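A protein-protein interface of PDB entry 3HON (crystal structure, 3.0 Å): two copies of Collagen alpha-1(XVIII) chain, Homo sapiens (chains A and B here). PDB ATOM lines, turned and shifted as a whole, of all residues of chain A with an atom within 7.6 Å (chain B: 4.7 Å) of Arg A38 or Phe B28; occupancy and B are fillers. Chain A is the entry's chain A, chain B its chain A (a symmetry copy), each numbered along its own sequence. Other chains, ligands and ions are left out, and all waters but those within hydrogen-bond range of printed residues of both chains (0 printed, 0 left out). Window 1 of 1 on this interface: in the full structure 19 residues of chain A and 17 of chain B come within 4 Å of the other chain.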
ATOM      1  N   SER A   3      11.395   9.068 -19.373  1.00  0.00           N
ATOM      2  CA  SER A   3      10.129   8.973 -20.088  1.00  0.00           C
ATOM      3  C   SER A   3       9.699  10.328 -20.634  1.00  0.00           C
ATOM      4  O   SER A   3      10.537  11.180 -20.946  1.00  0.00           O
ATOM      5  CB  SER A   3       9.042   8.439 -19.166  1.00  0.00           C
ATOM      6  OG  SER A   3       8.699   9.411 -18.199  1.00  0.00           O
ATOM      7  N   GLN A  17      -4.323   2.725 -27.706  1.00  0.00           N
ATOM      8  CA  GLN A  17      -2.888   2.922 -27.770  1.00  0.00           C
ATOM      9  C   GLN A  17      -2.179   2.989 -26.433  1.00  0.00           C
ATOM     10  O   GLN A  17      -0.970   3.187 -26.400  1.00  0.00           O
ATOM     11  CB  GLN A  17      -2.570   4.181 -28.557  1.00  0.00           C
ATOM     12  CG  GLN A  17      -2.735   3.999 -30.035  1.00  0.00           C
ATOM     13  CD  GLN A  17      -1.841   4.930 -30.820  1.00  0.00           C
ATOM     14  OE1 GLN A  17      -2.137   6.121 -30.964  1.00  0.00           O
ATOM     15  NE2 GLN A  17      -0.721   4.397 -31.320  1.00  0.00           N
ATOM     16  N   VAL A  18      -2.913   2.847 -25.333  1.00  0.00           N
ATOM     17  CA  VAL A  18      -2.287   2.876 -24.009  1.00  0.00           C
ATOM     18  C   VAL A  18      -1.494   1.576 -23.868  1.00  0.00           C
ATOM     19  O   VAL A  18      -0.752   1.370 -22.898  1.00  0.00           O
ATOM     20  CB  VAL A  18      -3.348   2.959 -22.877  1.00  0.00           C
ATOM     21  CG1 VAL A  18      -4.320   1.808 -23.004  1.00  0.00           C
ATOM     22  CG2 VAL A  18      -2.677   2.941 -21.504  1.00  0.00           C
ATOM     23  N   HIS A  19      -1.656   0.713 -24.869  1.00  0.00           N
ATOM     24  CA  HIS A  19      -1.004  -0.590 -24.919  1.00  0.00           C
ATOM     25  C   HIS A  19       0.508  -0.462 -25.115  1.00  0.00           C
ATOM     26  O   HIS A  19       1.281  -1.143 -24.434  1.00  0.00           O
ATOM     27  CB  HIS A  19      -1.664  -1.415 -26.029  1.00  0.00           C
ATOM     28  CG  HIS A  19      -3.159  -1.483 -25.907  1.00  0.00           C
ATOM     29  ND1 HIS A  19      -3.802  -2.363 -25.061  1.00  0.00           N
ATOM     30  CD2 HIS A  19      -4.133  -0.731 -26.477  1.00  0.00           C
ATOM     31  CE1 HIS A  19      -5.106  -2.150 -25.115  1.00  0.00           C
ATOM     32  NE2 HIS A  19      -5.333  -1.165 -25.965  1.00  0.00           N
ATOM     33  N   GLU A  20       0.923   0.417 -26.030  1.00  0.00           N
ATOM     34  CA  GLU A  20       2.350   0.658 -26.290  1.00  0.00           C
ATOM     35  C   GLU A  20       2.985   1.493 -25.170  1.00  0.00           C
ATOM     36  O   GLU A  20       3.741   0.967 -24.351  1.00  0.00           O
ATOM     37  CB  GLU A  20       2.561   1.388 -27.625  1.00  0.00           C
ATOM     38  CG  GLU A  20       2.506   0.519 -28.875  1.00  0.00           C
ATOM     39  CD  GLU A  20       1.206   0.681 -29.637  1.00  0.00           C
ATOM     40  OE1 GLU A  20       0.172   0.161 -29.159  1.00  0.00           O
ATOM     41  OE2 GLU A  20       1.225   1.338 -30.706  1.00  0.00           O
ATOM     42  N   VAL A  21       2.682   2.792 -25.152  1.00  0.00           N
ATOM     43  CA  VAL A  21       3.199   3.706 -24.132  1.00  0.00           C
ATOM     44  C   VAL A  21       3.649   2.946 -22.868  1.00  0.00           C
ATOM     45  O   VAL A  21       2.837   2.494 -22.054  1.00  0.00           O
ATOM     46  CB  VAL A  21       2.128   4.795 -23.769  1.00  0.00           C
ATOM     47  CG1 VAL A  21       0.856   4.146 -23.250  1.00  0.00           C
ATOM     48  CG2 VAL A  21       2.682   5.757 -22.740  1.00  0.00           C
ATOM     49  N   PRO A  22       4.969   2.787 -22.709  1.00  0.00           N
ATOM     50  CA  PRO A  22       5.649   2.101 -21.607  1.00  0.00           C
ATOM     51  C   PRO A  22       5.416   2.743 -20.249  1.00  0.00           C
ATOM     52  O   PRO A  22       5.008   3.899 -20.184  1.00  0.00           O
ATOM     53  CB  PRO A  22       7.106   2.175 -22.020  1.00  0.00           C
ATOM     54  CG  PRO A  22       7.165   3.503 -22.718  1.00  0.00           C
ATOM     55  CD  PRO A  22       5.949   3.436 -23.596  1.00  0.00           C
ATOM     56  N   GLU A  23       5.703   1.997 -19.176  1.00  0.00           N
ATOM     57  CA  GLU A  23       5.522   2.467 -17.797  1.00  0.00           C
ATOM     58  C   GLU A  23       6.087   3.850 -17.519  1.00  0.00           C
ATOM     59  O   GLU A  23       7.015   4.300 -18.173  1.00  0.00           O
ATOM     60  CB  GLU A  23       6.141   1.488 -16.805  1.00  0.00           C
ATOM     61  CG  GLU A  23       5.565   0.090 -16.882  1.00  0.00           C
ATOM     62  CD  GLU A  23       5.730  -0.700 -15.586  1.00  0.00           C
ATOM     63  OE1 GLU A  23       5.513  -1.933 -15.617  1.00  0.00           O
ATOM     64  OE2 GLU A  23       6.060  -0.094 -14.538  1.00  0.00           O
ATOM     65  N   GLY A  24       5.515   4.529 -16.538  1.00  0.00           N
ATOM     66  CA  GLY A  24       5.989   5.855 -16.201  1.00  0.00           C
ATOM     67  C   GLY A  24       5.928   6.877 -17.316  1.00  0.00           C
ATOM     68  O   GLY A  24       6.855   7.661 -17.495  1.00  0.00           O
ATOM     69  N   TRP A  25       4.843   6.879 -18.077  1.00  0.00           N
ATOM     70  CA  TRP A  25       4.696   7.852 -19.142  1.00  0.00           C
ATOM     71  C   TRP A  25       3.378   8.545 -18.978  1.00  0.00           C
ATOM     72  O   TRP A  25       2.341   7.925 -19.140  1.00  0.00           O
ATOM     73  CB  TRP A  25       4.712   7.181 -20.500  1.00  0.00           C
ATOM     74  CG  TRP A  25       6.045   7.068 -21.086  1.00  0.00           C
ATOM     75  CD1 TRP A  25       7.020   6.201 -20.727  1.00  0.00           C
ATOM     76  CD2 TRP A  25       6.569   7.849 -22.163  1.00  0.00           C
ATOM     77  NE1 TRP A  25       8.127   6.384 -21.518  1.00  0.00           N
ATOM     78  CE2 TRP A  25       7.875   7.391 -22.409  1.00  0.00           C
ATOM     79  CE3 TRP A  25       6.058   8.893 -22.946  1.00  0.00           C
ATOM     80  CZ2 TRP A  25       8.686   7.941 -23.412  1.00  0.00           C
ATOM     81  CZ3 TRP A  25       6.864   9.441 -23.942  1.00  0.00           C
ATOM     82  CH2 TRP A  25       8.162   8.961 -24.164  1.00  0.00           C
ATOM     83  N   LEU A  26       3.403   9.827 -18.645  1.00  0.00           N
ATOM     84  CA  LEU A  26       2.160  10.555 -18.485  1.00  0.00           C
ATOM     85  C   LEU A  26       1.383  10.419 -19.793  1.00  0.00           C
ATOM     86  O   LEU A  26       1.971  10.270 -20.868  1.00  0.00           O
ATOM     87  CB  LEU A  26       2.432  12.030 -18.167  1.00  0.00           C
ATOM     88  CG  LEU A  26       2.987  12.399 -16.793  1.00  0.00           C
ATOM     89  CD1 LEU A  26       2.055  11.932 -15.732  1.00  0.00           C
ATOM     90  CD2 LEU A  26       4.314  11.766 -16.595  1.00  0.00           C
ATOM     91  N   ILE A  27       0.059  10.464 -19.687  1.00  0.00           N
ATOM     92  CA  ILE A  27      -0.825  10.326 -20.835  1.00  0.00           C
ATOM     93  C   ILE A  27      -1.861  11.440 -20.821  1.00  0.00           C
ATOM     94  O   ILE A  27      -2.720  11.459 -19.949  1.00  0.00           O
ATOM     95  CB  ILE A  27      -1.542   8.960 -20.788  1.00  0.00           C
ATOM     96  CG1 ILE A  27      -0.525   7.839 -21.014  1.00  0.00           C
ATOM     97  CG2 ILE A  27      -2.626   8.899 -21.831  1.00  0.00           C
ATOM     98  CD1 ILE A  27      -1.038   6.459 -20.695  1.00  0.00           C
ATOM     99  N   LEU A  35      -5.231  13.784 -17.300  1.00  0.00           N
ATOM    100  CA  LEU A  35      -3.831  13.388 -17.259  1.00  0.00           C
ATOM    101  C   LEU A  35      -3.730  12.149 -16.383  1.00  0.00           C
ATOM    102  O   LEU A  35      -4.106  12.185 -15.216  1.00  0.00           O
ATOM    103  CB  LEU A  35      -2.953  14.501 -16.673  1.00  0.00           C
ATOM    104  CG  LEU A  35      -1.478  14.566 -17.108  1.00  0.00           C
ATOM    105  CD1 LEU A  35      -0.751  15.669 -16.384  1.00  0.00           C
ATOM    106  CD2 LEU A  35      -0.801  13.267 -16.820  1.00  0.00           C
ATOM    107  N   TYR A  36      -3.250  11.050 -16.967  1.00  0.00           N
ATOM    108  CA  TYR A  36      -3.065   9.794 -16.257  1.00  0.00           C
ATOM    109  C   TYR A  36      -1.604   9.464 -16.461  1.00  0.00           C
ATOM    110  O   TYR A  36      -0.980   9.966 -17.386  1.00  0.00           O
ATOM    111  CB  TYR A  36      -3.851   8.659 -16.899  1.00  0.00           C
ATOM    112  CG  TYR A  36      -5.238   8.973 -17.390  1.00  0.00           C
ATOM    113  CD1 TYR A  36      -6.362   8.537 -16.691  1.00  0.00           C
ATOM    114  CD2 TYR A  36      -5.429   9.655 -18.585  1.00  0.00           C
ATOM    115  CE1 TYR A  36      -7.641   8.767 -17.170  1.00  0.00           C
ATOM    116  CE2 TYR A  36      -6.701   9.892 -19.076  1.00  0.00           C
ATOM    117  CZ  TYR A  36      -7.803   9.446 -18.367  1.00  0.00           C
ATOM    118  OH  TYR A  36      -9.056   9.687 -18.875  1.00  0.00           O
ATOM    119  N   VAL A  37      -1.060   8.611 -15.606  1.00  0.00           N
ATOM    120  CA  VAL A  37       0.322   8.186 -15.741  1.00  0.00           C
ATOM    121  C   VAL A  37       0.255   6.680 -15.932  1.00  0.00           C
ATOM    122  O   VAL A  37      -0.473   6.004 -15.214  1.00  0.00           O
ATOM    123  CB  VAL A  37       1.139   8.508 -14.489  1.00  0.00           C
ATOM    124  CG1 VAL A  37       0.575   7.787 -13.294  1.00  0.00           C
ATOM    125  CG2 VAL A  37       2.568   8.109 -14.705  1.00  0.00           C
ATOM    126  N   ARG A  38       1.000   6.160 -16.905  1.00  0.00           N
ATOM    127  CA  ARG A  38       0.995   4.734 -17.220  1.00  0.00           C
ATOM    128  C   ARG A  38       1.692   3.917 -16.161  1.00  0.00           C
ATOM    129  O   ARG A  38       2.887   4.048 -15.980  1.00  0.00           O
ATOM    130  CB  ARG A  38       1.680   4.514 -18.554  1.00  0.00           C
ATOM    131  CG  ARG A  38       1.758   3.080 -18.966  1.00  0.00           C
ATOM    132  CD  ARG A  38       0.396   2.526 -19.274  1.00  0.00           C
ATOM    133  NE  ARG A  38       0.492   1.332 -20.110  1.00  0.00           N
ATOM    134  CZ  ARG A  38       0.759   0.109 -19.661  1.00  0.00           C
ATOM    135  NH1 ARG A  38       0.959  -0.110 -18.368  1.00  0.00           N
ATOM    136  NH2 ARG A  38       0.827  -0.897 -20.515  1.00  0.00           N
ATOM    137  N   VAL A  39       0.946   3.072 -15.461  1.00  0.00           N
ATOM    138  CA  VAL A  39       1.536   2.251 -14.406  1.00  0.00           C
ATOM    139  C   VAL A  39       1.677   0.778 -14.767  1.00  0.00           C
ATOM    140  O   VAL A  39       1.221   0.333 -15.825  1.00  0.00           O
ATOM    141  CB  VAL A  39       0.745   2.340 -13.052  1.00  0.00           C
ATOM    142  CG1 VAL A  39       1.187   3.553 -12.265  1.00  0.00           C
ATOM    143  CG2 VAL A  39      -0.752   2.382 -13.302  1.00  0.00           C
ATOM    144  N   GLN A  40       2.319   0.043 -13.856  1.00  0.00           N
ATOM    145  CA  GLN A  40       2.586  -1.388 -13.979  1.00  0.00           C
ATOM    146  C   GLN A  40       1.658  -2.182 -14.899  1.00  0.00           C
ATOM    147  O   GLN A  40       2.126  -2.793 -15.860  1.00  0.00           O
ATOM    148  CB  GLN A  40       2.603  -2.032 -12.584  1.00  0.00           C
ATOM    149  CG  GLN A  40       3.727  -1.521 -11.665  1.00  0.00           C
ATOM    150  CD  GLN A  40       4.003  -2.456 -10.483  1.00  0.00           C
ATOM    151  OE1 GLN A  40       3.117  -2.726  -9.671  1.00  0.00           O
ATOM    152  NE2 GLN A  40       5.238  -2.951 -10.386  1.00  0.00           N
ATOM    153  N   ASN A  41       0.355  -2.185 -14.618  1.00  0.00           N
ATOM    154  CA  ASN A  41      -0.582  -2.929 -15.461  1.00  0.00           C
ATOM    155  C   ASN A  41      -1.907  -2.203 -15.697  1.00  0.00           C
ATOM    156  O   ASN A  41      -2.972  -2.667 -15.280  1.00  0.00           O
ATOM    157  CB  ASN A  41      -0.859  -4.298 -14.853  1.00  0.00           C
ATOM    158  CG  ASN A  41      -1.496  -5.237 -15.835  1.00  0.00           C
ATOM    159  OD1 ASN A  41      -0.900  -5.566 -16.861  1.00  0.00           O
ATOM    160  ND2 ASN A  41      -2.716  -5.673 -15.540  1.00  0.00           N
ATOM    161  N   GLY A  42      -1.829  -1.079 -16.401  1.00  0.00           N
ATOM    162  CA  GLY A  42      -2.999  -0.261 -16.681  1.00  0.00           C
ATOM    163  C   GLY A  42      -2.603   1.160 -16.316  1.00  0.00           C
ATOM    164  O   GLY A  42      -1.423   1.401 -16.047  1.00  0.00           O
ATOM    165  N   PHE A  43      -3.540   2.102 -16.297  1.00  0.00           N
ATOM    166  CA  PHE A  43      -3.167   3.465 -15.949  1.00  0.00           C
ATOM    167  C   PHE A  43      -3.807   4.007 -14.666  1.00  0.00           C
ATOM    168  O   PHE A  43      -4.871   3.542 -14.266  1.00  0.00           O
ATOM    169  CB  PHE A  43      -3.420   4.421 -17.138  1.00  0.00           C
ATOM    170  CG  PHE A  43      -4.703   4.163 -17.906  1.00  0.00           C
ATOM    171  CD1 PHE A  43      -4.818   3.075 -18.770  1.00  0.00           C
ATOM    172  CD2 PHE A  43      -5.779   5.052 -17.813  1.00  0.00           C
ATOM    173  CE1 PHE A  43      -5.993   2.878 -19.539  1.00  0.00           C
ATOM    174  CE2 PHE A  43      -6.954   4.864 -18.573  1.00  0.00           C
ATOM    175  CZ  PHE A  43      -7.060   3.778 -19.438  1.00  0.00           C
ATOM    176  N   ARG A  44      -3.132   4.962 -14.011  1.00  0.00           N
ATOM    177  CA  ARG A  44      -3.618   5.609 -12.782  1.00  0.00           C
ATOM    178  C   ARG A  44      -3.786   7.112 -13.002  1.00  0.00           C
ATOM    179  O   ARG A  44      -2.823   7.864 -12.962  1.00  0.00           O
ATOM    180  CB  ARG A  44      -2.640   5.379 -11.632  1.00  0.00           C
ATOM    181  CG  ARG A  44      -2.726   3.998 -11.019  1.00  0.00           C
ATOM    182  CD  ARG A  44      -1.472   3.626 -10.220  1.00  0.00           C
ATOM    183  NE  ARG A  44      -1.581   3.731  -8.756  1.00  0.00           N
ATOM    184  CZ  ARG A  44      -1.800   4.861  -8.093  1.00  0.00           C
ATOM    185  NH1 ARG A  44      -1.952   5.995  -8.754  1.00  0.00           N
ATOM    186  NH2 ARG A  44      -1.815   4.860  -6.767  1.00  0.00           N
ATOM    187  N   LYS A  45      -5.020   7.540 -13.231  1.00  0.00           N
ATOM    188  CA  LYS A  45      -5.360   8.940 -13.490  1.00  0.00           C
ATOM    189  C   LYS A  45      -4.992   9.922 -12.395  1.00  0.00           C
ATOM    190  O   LYS A  45      -5.485   9.801 -11.283  1.00  0.00           O
ATOM    191  CB  LYS A  45      -6.858   9.011 -13.738  1.00  0.00           C
ATOM    192  CG  LYS A  45      -7.491  10.371 -13.718  1.00  0.00           C
ATOM    193  CD  LYS A  45      -8.967  10.161 -14.003  1.00  0.00           C
ATOM    194  CE  LYS A  45      -9.776  11.439 -13.915  1.00  0.00           C
ATOM    195  NZ  LYS A  45     -11.241  11.170 -14.113  1.00  0.00           N
ATOM    196  N   VAL B   5      10.710  13.465 -16.932  1.00  0.00           N
ATOM    197  CA  VAL B   5      10.232  12.475 -15.950  1.00  0.00           C
ATOM    198  C   VAL B   5      11.310  11.405 -15.805  1.00  0.00           C
ATOM    199  O   VAL B   5      11.815  10.892 -16.804  1.00  0.00           O
ATOM    200  CB  VAL B   5       8.911  11.793 -16.411  1.00  0.00           C
ATOM    201  CG1 VAL B   5       8.501  10.704 -15.439  1.00  0.00           C
ATOM    202  CG2 VAL B   5       7.819  12.821 -16.514  1.00  0.00           C
ATOM    203  N   ARG B   6      11.675  11.074 -14.573  1.00  0.00           N
ATOM    204  CA  ARG B   6      12.705  10.067 -14.373  1.00  0.00           C
ATOM    205  C   ARG B   6      12.166   8.750 -13.832  1.00  0.00           C
ATOM    206  O   ARG B   6      11.582   8.707 -12.753  1.00  0.00           O
ATOM    207  CB  ARG B   6      13.798  10.613 -13.460  1.00  0.00           C
ATOM    208  CG  ARG B   6      14.616  11.719 -14.101  1.00  0.00           C
ATOM    209  CD  ARG B   6      16.075  11.624 -13.690  1.00  0.00           C
ATOM    210  NE  ARG B   6      16.627  10.298 -13.979  1.00  0.00           N
ATOM    211  CZ  ARG B   6      17.893   9.940 -13.764  1.00  0.00           C
ATOM    212  NH1 ARG B   6      18.758  10.815 -13.257  1.00  0.00           N
ATOM    213  NH2 ARG B   6      18.294   8.706 -14.054  1.00  0.00           N
ATOM    214  N   LEU B   7      12.381   7.681 -14.599  1.00  0.00           N
ATOM    215  CA  LEU B   7      11.921   6.339 -14.249  1.00  0.00           C
ATOM    216  C   LEU B   7      12.810   5.586 -13.252  1.00  0.00           C
ATOM    217  O   LEU B   7      14.038   5.671 -13.305  1.00  0.00           O
ATOM    218  CB  LEU B   7      11.782   5.490 -15.514  1.00  0.00           C
ATOM    219  CG  LEU B   7      10.859   5.995 -16.617  1.00  0.00           C
ATOM    220  CD1 LEU B   7      10.845   5.017 -17.789  1.00  0.00           C
ATOM    221  CD2 LEU B   7       9.479   6.172 -16.044  1.00  0.00           C
ATOM    222  N   TRP B   8      12.163   4.838 -12.357  1.00  0.00           N
ATOM    223  CA  TRP B   8      12.834   4.030 -11.339  1.00  0.00           C
ATOM    224  C   TRP B   8      12.136   2.677 -11.133  1.00  0.00           C
ATOM    225  O   TRP B   8      10.960   2.520 -11.461  1.00  0.00           O
ATOM    226  CB  TRP B   8      12.905   4.799 -10.018  1.00  0.00           C
ATOM    227  CG  TRP B   8      14.150   5.615  -9.905  1.00  0.00           C
ATOM    228  CD1 TRP B   8      15.421   5.144  -9.770  1.00  0.00           C
ATOM    229  CD2 TRP B   8      14.259   7.042  -9.991  1.00  0.00           C
ATOM    230  NE1 TRP B   8      16.317   6.184  -9.773  1.00  0.00           N
ATOM    231  CE2 TRP B   8      15.631   7.361  -9.908  1.00  0.00           C
ATOM    232  CE3 TRP B   8      13.329   8.082 -10.134  1.00  0.00           C
ATOM    233  CZ2 TRP B   8      16.100   8.680  -9.963  1.00  0.00           C
ATOM    234  CZ3 TRP B   8      13.794   9.397 -10.189  1.00  0.00           C
ATOM    235  CH2 TRP B   8      15.169   9.682 -10.103  1.00  0.00           C
ATOM    236  N   LEU B  26       9.498  15.325 -12.585  1.00  0.00           N
ATOM    237  CA  LEU B  26       8.649  14.266 -12.078  1.00  0.00           C
ATOM    238  C   LEU B  26       9.549  13.070 -11.772  1.00  0.00           C
ATOM    239  O   LEU B  26      10.595  12.885 -12.401  1.00  0.00           O
ATOM    240  CB  LEU B  26       7.578  13.888 -13.108  1.00  0.00           C
ATOM    241  CG  LEU B  26       6.436  14.865 -13.377  1.00  0.00           C
ATOM    242  CD1 LEU B  26       5.693  15.131 -12.116  1.00  0.00           C
ATOM    243  CD2 LEU B  26       6.974  16.141 -13.909  1.00  0.00           C
ATOM    244  N   ILE B  27       9.135  12.268 -10.797  1.00  0.00           N
ATOM    245  CA  ILE B  27       9.889  11.100 -10.368  1.00  0.00           C
ATOM    246  C   ILE B  27       8.966   9.892 -10.292  1.00  0.00           C
ATOM    247  O   ILE B  27       8.091   9.850  -9.437  1.00  0.00           O
ATOM    248  CB  ILE B  27      10.513  11.355  -8.979  1.00  0.00           C
ATOM    249  CG1 ILE B  27      11.598  12.428  -9.093  1.00  0.00           C
ATOM    250  CG2 ILE B  27      11.094  10.081  -8.422  1.00  0.00           C
ATOM    251  CD1 ILE B  27      12.069  12.979  -7.773  1.00  0.00           C
ATOM    252  N   PHE B  28       9.169   8.910 -11.169  1.00  0.00           N
ATOM    253  CA  PHE B  28       8.327   7.719 -11.185  1.00  0.00           C
ATOM    254  C   PHE B  28       8.926   6.446 -10.561  1.00  0.00           C
ATOM    255  O   PHE B  28       9.886   5.882 -11.072  1.00  0.00           O
ATOM    256  CB  PHE B  28       7.889   7.420 -12.621  1.00  0.00           C
ATOM    257  CG  PHE B  28       6.968   6.234 -12.737  1.00  0.00           C
ATOM    258  CD1 PHE B  28       5.778   6.187 -12.020  1.00  0.00           C
ATOM    259  CD2 PHE B  28       7.286   5.160 -13.553  1.00  0.00           C
ATOM    260  CE1 PHE B  28       4.921   5.086 -12.114  1.00  0.00           C
ATOM    261  CE2 PHE B  28       6.433   4.060 -13.650  1.00  0.00           C
ATOM    262  CZ  PHE B  28       5.251   4.029 -12.930  1.00  0.00           C
ATOM    263  N   VAL B  29       8.345   5.986  -9.457  1.00  0.00           N
ATOM    264  CA  VAL B  29       8.817   4.768  -8.802  1.00  0.00           C
ATOM    265  C   VAL B  29       7.931   3.593  -9.265  1.00  0.00           C
ATOM    266  O   VAL B  29       7.127   3.054  -8.502  1.00  0.00           O
ATOM    267  CB  VAL B  29       8.743   4.904  -7.262  1.00  0.00           C
ATOM    268  CG1 VAL B  29       9.459   3.741  -6.597  1.00  0.00           C
ATOM    269  CG2 VAL B  29       9.364   6.212  -6.827  1.00  0.00           C
ATOM    270  N   ALA B  30       8.105   3.212 -10.530  1.00  0.00           N
ATOM    271  CA  ALA B  30       7.360   2.137 -11.201  1.00  0.00           C
ATOM    272  C   ALA B  30       6.785   0.986 -10.382  1.00  0.00           C
ATOM    273  O   ALA B  30       5.599   0.677 -10.496  1.00  0.00           O
ATOM    274  CB  ALA B  30       8.212   1.561 -12.334  1.00  0.00           C
ATOM    275  N   GLU B  33       4.289   2.400  -8.198  1.00  0.00           N
ATOM    276  CA  GLU B  33       3.248   3.105  -8.944  1.00  0.00           C
ATOM    277  C   GLU B  33       3.026   4.461  -8.286  1.00  0.00           C
ATOM    278  O   GLU B  33       1.887   4.877  -8.067  1.00  0.00           O
ATOM    279  CB  GLU B  33       1.945   2.296  -8.942  1.00  0.00           C
ATOM    280  CG  GLU B  33       2.055   0.909  -9.570  1.00  0.00           C
ATOM    281  CD  GLU B  33       0.763   0.132  -9.467  1.00  0.00           C
ATOM    282  OE1 GLU B  33      -0.174   0.400 -10.246  1.00  0.00           O
ATOM    283  OE2 GLU B  33       0.682  -0.741  -8.586  1.00  0.00           O
ATOM    284  N   GLU B  34       4.135   5.137  -7.982  1.00  0.00           N
ATOM    285  CA  GLU B  34       4.120   6.445  -7.323  1.00  0.00           C
ATOM    286  C   GLU B  34       4.767   7.520  -8.172  1.00  0.00           C
ATOM    287  O   GLU B  34       5.867   7.325  -8.676  1.00  0.00           O
ATOM    288  CB  GLU B  34       4.867   6.375  -5.986  1.00  0.00           C
ATOM    289  CG  GLU B  34       4.195   5.535  -4.911  1.00  0.00           C
ATOM    290  CD  GLU B  34       3.148   6.306  -4.140  1.00  0.00           C
ATOM    291  OE1 GLU B  34       2.244   6.895  -4.772  1.00  0.00           O
ATOM    292  OE2 GLU B  34       3.230   6.316  -2.895  1.00  0.00           O
ATOM    293  N   LEU B  54      -5.782  -2.229 -18.130  1.00  0.00           N
ATOM    294  CA  LEU B  54      -5.180  -1.959 -19.439  1.00  0.00           C
ATOM    295  C   LEU B  54      -5.710  -2.764 -20.653  1.00  0.00           C
ATOM    296  O   LEU B  54      -6.095  -2.168 -21.675  1.00  0.00           O
ATOM    297  CB  LEU B  54      -3.664  -2.162 -19.336  1.00  0.00           C
ATOM    298  CG  LEU B  54      -2.840  -1.899 -20.593  1.00  0.00           C
ATOM    299  CD1 LEU B  54      -2.294  -0.484 -20.540  1.00  0.00           C
ATOM    300  CD2 LEU B  54      -1.703  -2.907 -20.684  1.00  0.00           C
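Positions printed for both chains: 26 and 27. Of the 17 pairs that touch across the chains among the printed residues, none has its exchanged pair printed and touching as well.
The backbone carbonyl oxygen (O) of Val A18 is in hydrogen-bond range of the guanidinium group (NE) of Arg A38, 3.1 Å away. The backbone carbonyl oxygen (O) of Val A21 lies within hydrogen-bond range of the guanidinium group (NE) of Arg A38, 3.3 Å away. N of Arg A38 lies within hydrogen-bond range of O of Trp A25 (3.1 Å). The backbone NH (N) of Arg A44 is in hydrogen-bond range of the backbone carbonyl oxygen (O) of Val A37, at 3.1 Å. The backbone NH of Phe B28 lies within hydrogen-bond range of the backbone carbonyl oxygen of Arg B6, 2.9 Å away. The backbone NH of Ala B30 sits close to the backbone carbonyl oxygen of Trp B8, at 3.1 Å.
Among the printed residues, pairs that only touch across the chains: Ser A3 with Leu B7, Val A18 with Leu B54, His A19 with Leu B54, Glu A23 with Leu B7, Glu A23 with Phe B28, Glu A23 with Ala B30, Gly A24 with Leu B7, Gly A24 with Phe B28, Leu A26 with Val B5, Arg A38 with Phe B28, Arg A38 with Leu B54, Val A39 with Glu B33, Gln A40 with Ala B30 and Gly A42 with Leu B54.
Val A21 touches none of the printed residues of chain B. Printed residues of chain B within 4 Å of Glu A23: Leu B7 (3.8 Å), Phe B28 (3.9 Å) and Ala B30 (3.5 Å). Arg A38 touches two residues of chain B. Of the printed residues of chain B, Val A39 touches Glu B33. Printed residues of chain B within 4 Å of Arg A44: Glu B33. Of the printed residues of chain A, Leu B7 touches Ser A3, Glu A23 and Gly A24. Of chain A, only Glu A23 (3.9 Å), Gly A24 (3.0 Å) and Arg A38 (3.9 Å) come within 4 Å of Phe B28. Of the printed residues of chain A, Ala B30 touches Glu A23 and Gln A40. The nearest printed residue of chain B that does not touch Arg A38 is Ala B30 (6.8 Å).
The backbone carbonyl oxygen (O) of Val B5 sits at hydrogen-bond distance from the backbone NH (N) of Ser A3, at 3.2 Å. The side-chain amide oxygen (OE1) of Gln A40 lies close to the side-chain carboxylate (OE2) of Glu B33 (3.3 Å). OE1 of Glu B33 is in salt-bridge range of NE of Arg A44, at 3.9 Å.
Among the printed residues, Asp or Glu carboxylates within 4 Å of a Lys or Arg side-chain nitrogen of the other chain: Arg A44 with Glu B33.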
